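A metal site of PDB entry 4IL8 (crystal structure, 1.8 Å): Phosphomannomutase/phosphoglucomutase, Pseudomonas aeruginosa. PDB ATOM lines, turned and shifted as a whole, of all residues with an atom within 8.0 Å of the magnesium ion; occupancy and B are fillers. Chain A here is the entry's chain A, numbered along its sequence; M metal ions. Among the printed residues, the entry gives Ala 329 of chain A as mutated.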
ATOM      1  N   ASP A  56     -20.766  24.588  -2.042  1.00  0.00           N
ATOM      2  CA  ASP A  56     -20.865  23.976  -3.365  1.00  0.00           C
ATOM      3  C   ASP A  56     -22.357  23.887  -3.818  1.00  0.00           C
ATOM      4  O   ASP A  56     -23.201  24.610  -3.249  1.00  0.00           O
ATOM      5  CB  ASP A  56     -20.094  22.641  -3.455  1.00  0.00           C
ATOM      6  CG  ASP A  56     -20.771  21.494  -2.685  1.00  0.00           C
ATOM      7  OD1 ASP A  56     -21.926  21.672  -2.208  1.00  0.00           O
ATOM      8  OD2 ASP A  56     -20.170  20.404  -2.635  1.00  0.00           O
ATOM      9  N   THR A  87     -14.826  25.310  -4.646  1.00  0.00           N
ATOM     10  CA  THR A  87     -13.847  25.306  -3.573  1.00  0.00           C
ATOM     11  C   THR A  87     -12.631  26.228  -3.836  1.00  0.00           C
ATOM     12  O   THR A  87     -12.265  26.992  -2.937  1.00  0.00           O
ATOM     13  CB  THR A  87     -13.409  23.848  -3.237  1.00  0.00           C
ATOM     14  OG1 THR A  87     -14.559  23.142  -2.685  1.00  0.00           O
ATOM     15  CG2 THR A  87     -12.206  23.820  -2.235  1.00  0.00           C
ATOM     16  N   PRO A  88     -11.965  26.156  -5.029  1.00  0.00           N
ATOM     17  CA  PRO A  88     -10.774  27.036  -5.138  1.00  0.00           C
ATOM     18  C   PRO A  88     -11.147  28.535  -5.139  1.00  0.00           C
ATOM     19  O   PRO A  88     -10.281  29.394  -4.915  1.00  0.00           O
ATOM     20  CB  PRO A  88     -10.155  26.654  -6.509  1.00  0.00           C
ATOM     21  CG  PRO A  88     -11.302  25.949  -7.277  1.00  0.00           C
ATOM     22  CD  PRO A  88     -12.089  25.241  -6.171  1.00  0.00           C
ATOM     23  N   TYR A  91     -11.044  29.332  -1.535  1.00  0.00           N
ATOM     24  CA  TYR A  91      -9.603  29.473  -1.185  1.00  0.00           C
ATOM     25  C   TYR A  91      -9.060  30.808  -1.687  1.00  0.00           C
ATOM     26  O   TYR A  91      -8.253  31.448  -1.010  1.00  0.00           O
ATOM     27  CB  TYR A  91      -8.755  28.361  -1.799  1.00  0.00           C
ATOM     28  CG  TYR A  91      -8.982  26.957  -1.251  1.00  0.00           C
ATOM     29  CD1 TYR A  91      -8.643  25.846  -2.032  1.00  0.00           C
ATOM     30  CD2 TYR A  91      -9.528  26.734   0.036  1.00  0.00           C
ATOM     31  CE1 TYR A  91      -8.813  24.542  -1.522  1.00  0.00           C
ATOM     32  CE2 TYR A  91      -9.702  25.442   0.534  1.00  0.00           C
ATOM     33  CZ  TYR A  91      -9.349  24.352  -0.246  1.00  0.00           C
ATOM     34  OH  TYR A  91      -9.538  23.057   0.218  1.00  0.00           O
ATOM     35  N   THR A 106     -18.560  21.701   1.556  1.00  0.00           N
ATOM     36  CA  THR A 106     -18.543  20.854   0.384  1.00  0.00           C
ATOM     37  C   THR A 106     -18.513  19.365   0.714  1.00  0.00           C
ATOM     38  O   THR A 106     -17.936  18.973   1.720  1.00  0.00           O
ATOM     39  CB  THR A 106     -17.330  21.195  -0.566  1.00  0.00           C
ATOM     40  OG1 THR A 106     -17.366  20.328  -1.691  1.00  0.00           O
ATOM     41  CG2 THR A 106     -15.962  21.068   0.135  1.00  0.00           C
ATOM     42  N   GLY A 107     -19.148  18.557  -0.132  1.00  0.00           N
ATOM     43  CA  GLY A 107     -19.007  17.097  -0.086  1.00  0.00           C
ATOM     44  C   GLY A 107     -18.188  16.585  -1.268  1.00  0.00           C
ATOM     45  O   GLY A 107     -18.176  15.381  -1.566  1.00  0.00           O
ATOM     46  N   SEP A 108     -17.549  17.525  -1.974  1.00  0.00           N
ATOM     47  CA  SEP A 108     -16.570  17.236  -3.047  1.00  0.00           C
ATOM     48  CB  SEP A 108     -15.306  16.627  -2.442  1.00  0.00           C
ATOM     49  OG  SEP A 108     -14.272  16.440  -3.411  1.00  0.00           O
ATOM     50  C   SEP A 108     -17.174  16.399  -4.190  1.00  0.00           C
ATOM     51  O   SEP A 108     -18.025  16.885  -4.927  1.00  0.00           O
ATOM     52  P   SEP A 108     -12.845  16.083  -2.736  1.00  0.00           P
ATOM     53  O1P SEP A 108     -12.547  14.514  -2.700  1.00  0.00           O
ATOM     54  O2P SEP A 108     -12.761  16.600  -1.205  1.00  0.00           O
ATOM     55  O3P SEP A 108     -11.680  16.786  -3.613  1.00  0.00           O
ATOM     56  N   HIS A 109     -16.753  15.133  -4.325  1.00  0.00           N
ATOM     57  CA  HIS A 109     -17.215  14.252  -5.402  1.00  0.00           C
ATOM     58  C   HIS A 109     -18.167  13.141  -4.911  1.00  0.00           C
ATOM     59  O   HIS A 109     -18.607  12.306  -5.717  1.00  0.00           O
ATOM     60  CB  HIS A 109     -16.005  13.635  -6.119  1.00  0.00           C
ATOM     61  CG  HIS A 109     -15.137  12.808  -5.218  1.00  0.00           C
ATOM     62  ND1 HIS A 109     -14.175  13.349  -4.408  1.00  0.00           N
ATOM     63  CD2 HIS A 109     -15.131  11.470  -4.977  1.00  0.00           C
ATOM     64  CE1 HIS A 109     -13.589  12.389  -3.709  1.00  0.00           C
ATOM     65  NE2 HIS A 109     -14.149  11.237  -4.035  1.00  0.00           N
ATOM     66  N   ASN A 110     -18.474  13.141  -3.610  1.00  0.00           N
ATOM     67  CA  ASN A 110     -19.344  12.118  -3.003  1.00  0.00           C
ATOM     68  C   ASN A 110     -20.808  12.153  -3.460  1.00  0.00           C
ATOM     69  O   ASN A 110     -21.248  13.145  -4.063  1.00  0.00           O
ATOM     70  CB  ASN A 110     -19.237  12.178  -1.483  1.00  0.00           C
ATOM     71  CG  ASN A 110     -17.817  12.004  -0.999  1.00  0.00           C
ATOM     72  OD1 ASN A 110     -17.204  10.971  -1.216  1.00  0.00           O
ATOM     73  ND2 ASN A 110     -17.283  13.023  -0.336  1.00  0.00           N
ATOM     74  N   LYS A 118     -14.102  22.032   4.311  1.00  0.00           N
ATOM     75  CA  LYS A 118     -12.661  22.200   4.190  1.00  0.00           C
ATOM     76  C   LYS A 118     -12.320  23.530   4.827  1.00  0.00           C
ATOM     77  O   LYS A 118     -13.034  24.523   4.651  1.00  0.00           O
ATOM     78  CB  LYS A 118     -12.243  22.123   2.726  1.00  0.00           C
ATOM     79  CG  LYS A 118     -12.421  20.686   2.166  1.00  0.00           C
ATOM     80  CD  LYS A 118     -12.171  20.653   0.680  1.00  0.00           C
ATOM     81  CE  LYS A 118     -12.481  19.259   0.156  1.00  0.00           C
ATOM     82  NZ  LYS A 118     -11.243  18.384   0.176  1.00  0.00           N
ATOM     83  N   PRO A 215     -19.852  13.831 -10.389  1.00  0.00           N
ATOM     84  CA  PRO A 215     -18.670  14.595 -10.826  1.00  0.00           C
ATOM     85  C   PRO A 215     -17.376  14.100 -10.130  1.00  0.00           C
ATOM     86  O   PRO A 215     -16.885  14.710  -9.176  1.00  0.00           O
ATOM     87  CB  PRO A 215     -19.028  16.041 -10.424  1.00  0.00           C
ATOM     88  CG  PRO A 215     -19.957  15.865  -9.231  1.00  0.00           C
ATOM     89  CD  PRO A 215     -20.753  14.635  -9.528  1.00  0.00           C
ATOM     90  N   PRO A 217     -13.972  12.740 -11.858  1.00  0.00           N
ATOM     91  CA  PRO A 217     -13.210  12.330 -13.042  1.00  0.00           C
ATOM     92  C   PRO A 217     -12.092  11.336 -12.703  1.00  0.00           C
ATOM     93  O   PRO A 217     -11.369  10.908 -13.604  1.00  0.00           O
ATOM     94  CB  PRO A 217     -12.668  13.648 -13.607  1.00  0.00           C
ATOM     95  CG  PRO A 217     -12.576  14.578 -12.387  1.00  0.00           C
ATOM     96  CD  PRO A 217     -13.589  14.091 -11.370  1.00  0.00           C
ATOM     97  N   PHE A 241     -14.405  18.243 -14.622  1.00  0.00           N
ATOM     98  CA  PHE A 241     -14.170  18.797 -13.264  1.00  0.00           C
ATOM     99  C   PHE A 241     -14.835  17.935 -12.199  1.00  0.00           C
ATOM    100  O   PHE A 241     -15.884  17.348 -12.453  1.00  0.00           O
ATOM    101  CB  PHE A 241     -14.660  20.241 -13.194  1.00  0.00           C
ATOM    102  CG  PHE A 241     -13.891  21.150 -14.090  1.00  0.00           C
ATOM    103  CD1 PHE A 241     -12.600  21.562 -13.726  1.00  0.00           C
ATOM    104  CD2 PHE A 241     -14.406  21.547 -15.319  1.00  0.00           C
ATOM    105  CE1 PHE A 241     -11.847  22.373 -14.593  1.00  0.00           C
ATOM    106  CE2 PHE A 241     -13.653  22.368 -16.185  1.00  0.00           C
ATOM    107  CZ  PHE A 241     -12.376  22.780 -15.817  1.00  0.00           C
ATOM    108  N   ASP A 242     -14.246  17.834 -11.016  1.00  0.00           N
ATOM    109  CA  ASP A 242     -14.961  17.161  -9.929  1.00  0.00           C
ATOM    110  C   ASP A 242     -16.020  18.102  -9.385  1.00  0.00           C
ATOM    111  O   ASP A 242     -16.166  19.219  -9.890  1.00  0.00           O
ATOM    112  CB  ASP A 242     -14.041  16.524  -8.862  1.00  0.00           C
ATOM    113  CG  ASP A 242     -13.478  17.526  -7.874  1.00  0.00           C
ATOM    114  OD1 ASP A 242     -13.363  18.710  -8.253  1.00  0.00           O
ATOM    115  OD2 ASP A 242     -13.150  17.123  -6.724  1.00  0.00           O
ATOM    116  N   GLY A 243     -16.770  17.643  -8.394  1.00  0.00           N
ATOM    117  CA  GLY A 243     -17.967  18.341  -7.962  1.00  0.00           C
ATOM    118  C   GLY A 243     -17.755  19.737  -7.450  1.00  0.00           C
ATOM    119  O   GLY A 243     -18.597  20.595  -7.672  1.00  0.00           O
ATOM    120  N   ASP A 244     -16.624  19.950  -6.773  1.00  0.00           N
ATOM    121  CA  ASP A 244     -16.360  21.279  -6.185  1.00  0.00           C
ATOM    122  C   ASP A 244     -15.224  22.031  -6.902  1.00  0.00           C
ATOM    123  O   ASP A 244     -14.856  23.142  -6.535  1.00  0.00           O
ATOM    124  CB  ASP A 244     -16.205  21.145  -4.666  1.00  0.00           C
ATOM    125  CG  ASP A 244     -14.956  20.391  -4.244  1.00  0.00           C
ATOM    126  OD1 ASP A 244     -14.442  20.615  -3.108  1.00  0.00           O
ATOM    127  OD2 ASP A 244     -14.506  19.526  -5.024  1.00  0.00           O
ATOM    128  N   GLY A 245     -14.664  21.435  -7.938  1.00  0.00           N
ATOM    129  CA  GLY A 245     -13.720  22.153  -8.792  1.00  0.00           C
ATOM    130  C   GLY A 245     -12.250  22.205  -8.408  1.00  0.00           C
ATOM    131  O   GLY A 245     -11.479  22.946  -9.041  1.00  0.00           O
ATOM    132  N   ASP A 246     -11.833  21.424  -7.404  1.00  0.00           N
ATOM    133  CA  ASP A 246     -10.415  21.434  -7.061  1.00  0.00           C
ATOM    134  C   ASP A 246      -9.595  20.386  -7.833  1.00  0.00           C
ATOM    135  O   ASP A 246      -8.367  20.368  -7.707  1.00  0.00           O
ATOM    136  CB  ASP A 246     -10.128  21.394  -5.549  1.00  0.00           C
ATOM    137  CG  ASP A 246     -10.842  20.297  -4.826  1.00  0.00           C
ATOM    138  OD1 ASP A 246     -11.321  19.340  -5.490  1.00  0.00           O
ATOM    139  OD2 ASP A 246     -10.949  20.395  -3.548  1.00  0.00           O
ATOM    140  N   ARG A 247     -10.293  19.554  -8.616  1.00  0.00           N
ATOM    141  CA  ARG A 247      -9.633  18.501  -9.416  1.00  0.00           C
ATOM    142  C   ARG A 247     -10.117  18.576 -10.862  1.00  0.00           C
ATOM    143  O   ARG A 247     -11.244  19.038 -11.153  1.00  0.00           O
ATOM    144  CB  ARG A 247      -9.905  17.104  -8.810  1.00  0.00           C
ATOM    145  CG  ARG A 247      -9.405  16.953  -7.346  1.00  0.00           C
ATOM    146  CD  ARG A 247      -9.521  15.528  -6.793  1.00  0.00           C
ATOM    147  NE  ARG A 247     -10.884  15.008  -6.796  1.00  0.00           N
ATOM    148  CZ  ARG A 247     -11.261  13.856  -7.356  1.00  0.00           C
ATOM    149  NH1 ARG A 247     -10.379  13.080  -7.961  1.00  0.00           N
ATOM    150  NH2 ARG A 247     -12.532  13.480  -7.308  1.00  0.00           N
ATOM    151  N   VAL A 248      -9.248  18.155 -11.792  1.00  0.00           N
ATOM    152  CA  VAL A 248      -9.586  18.216 -13.212  1.00  0.00           C
ATOM    153  C   VAL A 248      -9.104  16.918 -13.875  1.00  0.00           C
ATOM    154  O   VAL A 248      -8.083  16.334 -13.448  1.00  0.00           O
ATOM    155  CB  VAL A 248      -8.948  19.473 -13.875  1.00  0.00           C
ATOM    156  CG1 VAL A 248      -7.399  19.434 -13.783  1.00  0.00           C
ATOM    157  CG2 VAL A 248      -9.410  19.656 -15.296  1.00  0.00           C
ATOM    158  N   SER A 327      -4.763  12.222  -7.481  1.00  0.00           N
ATOM    159  CA  SER A 327      -6.202  12.510  -7.392  1.00  0.00           C
ATOM    160  C   SER A 327      -6.678  13.451  -8.481  1.00  0.00           C
ATOM    161  O   SER A 327      -7.885  13.543  -8.769  1.00  0.00           O
ATOM    162  CB  SER A 327      -6.505  13.118  -6.018  1.00  0.00           C
ATOM    163  OG  SER A 327      -5.987  14.468  -5.959  1.00  0.00           O
ATOM    164  N   ALA A 329      -5.650  16.776  -8.225  1.00  0.00           N
ATOM    165  CA  ALA A 329      -5.449  18.117  -7.647  1.00  0.00           C
ATOM    166  C   ALA A 329      -4.083  18.662  -8.102  1.00  0.00           C
ATOM    167  O   ALA A 329      -3.047  17.990  -7.936  1.00  0.00           O
ATOM    168  CB  ALA A 329      -5.522  18.042  -6.124  1.00  0.00           C
ATOM    169  N   ASP A 340      -4.926  24.094  -4.511  1.00  0.00           N
ATOM    170  CA  ASP A 340      -5.413  23.185  -5.550  1.00  0.00           C
ATOM    171  C   ASP A 340      -6.629  23.834  -6.248  1.00  0.00           C
ATOM    172  O   ASP A 340      -7.533  24.388  -5.609  1.00  0.00           O
ATOM    173  CB  ASP A 340      -5.726  21.788  -4.993  1.00  0.00           C
ATOM    174  CG  ASP A 340      -6.404  21.825  -3.589  1.00  0.00           C
ATOM    175  OD1 ASP A 340      -7.209  20.893  -3.315  1.00  0.00           O
ATOM    176  OD2 ASP A 340      -6.141  22.723  -2.747  1.00  0.00           O
HETATM  177 MG    MG M   1     -12.921  18.061  -4.859  1.00  0.00          MG
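N of Arg 247 is in hydrogen-bond range of OD1 of Asp 242 (3.2 Å). The backbone NH (N) of Gly 245 lies within hydrogen-bond range of the side-chain carboxylate (OD1) of Asp 242 (3.0 Å). The side-chain carboxylate (OD1) of Asp 244 is in hydrogen-bond range of the side-chain hydroxyl (OG1) of Thr 87 (2.6 Å). The side-chain carboxylate of Asp 244 is in hydrogen-bond range of the side-chain hydroxyl of Thr 106 (3.3 Å). The guanidinium group of Arg 247 lies close to O3P of SEP 108 (3.7 Å). O1P of SEP 108 lies close to ND1 of His 109 (2.6 Å). O2P of SEP 108 lies within salt-bridge range of NZ of Lys 118, 2.7 Å away. N of SEP 108 lies within hydrogen-bond range of the side-chain hydroxyl (OG1) of Thr 106, at 2.8 Å.
Four residues have an atom within 4 Å of the magnesium ion: SEP 108, Asp 242, Asp 244 and Asp 246.
OD2 of Asp 242 binds the magnesium ion (2.1 Å). The magnesium ion is bound by OD1 of Asp 246 (2.1 Å). The magnesium ion is bound by the side-chain carboxylate (OD2) of Asp 244 (2.2 Å). O3P of SEP 108 is bound to the magnesium ion (2.2 Å). OG of SEP 108 binds the magnesium ion, at 2.6 Å.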
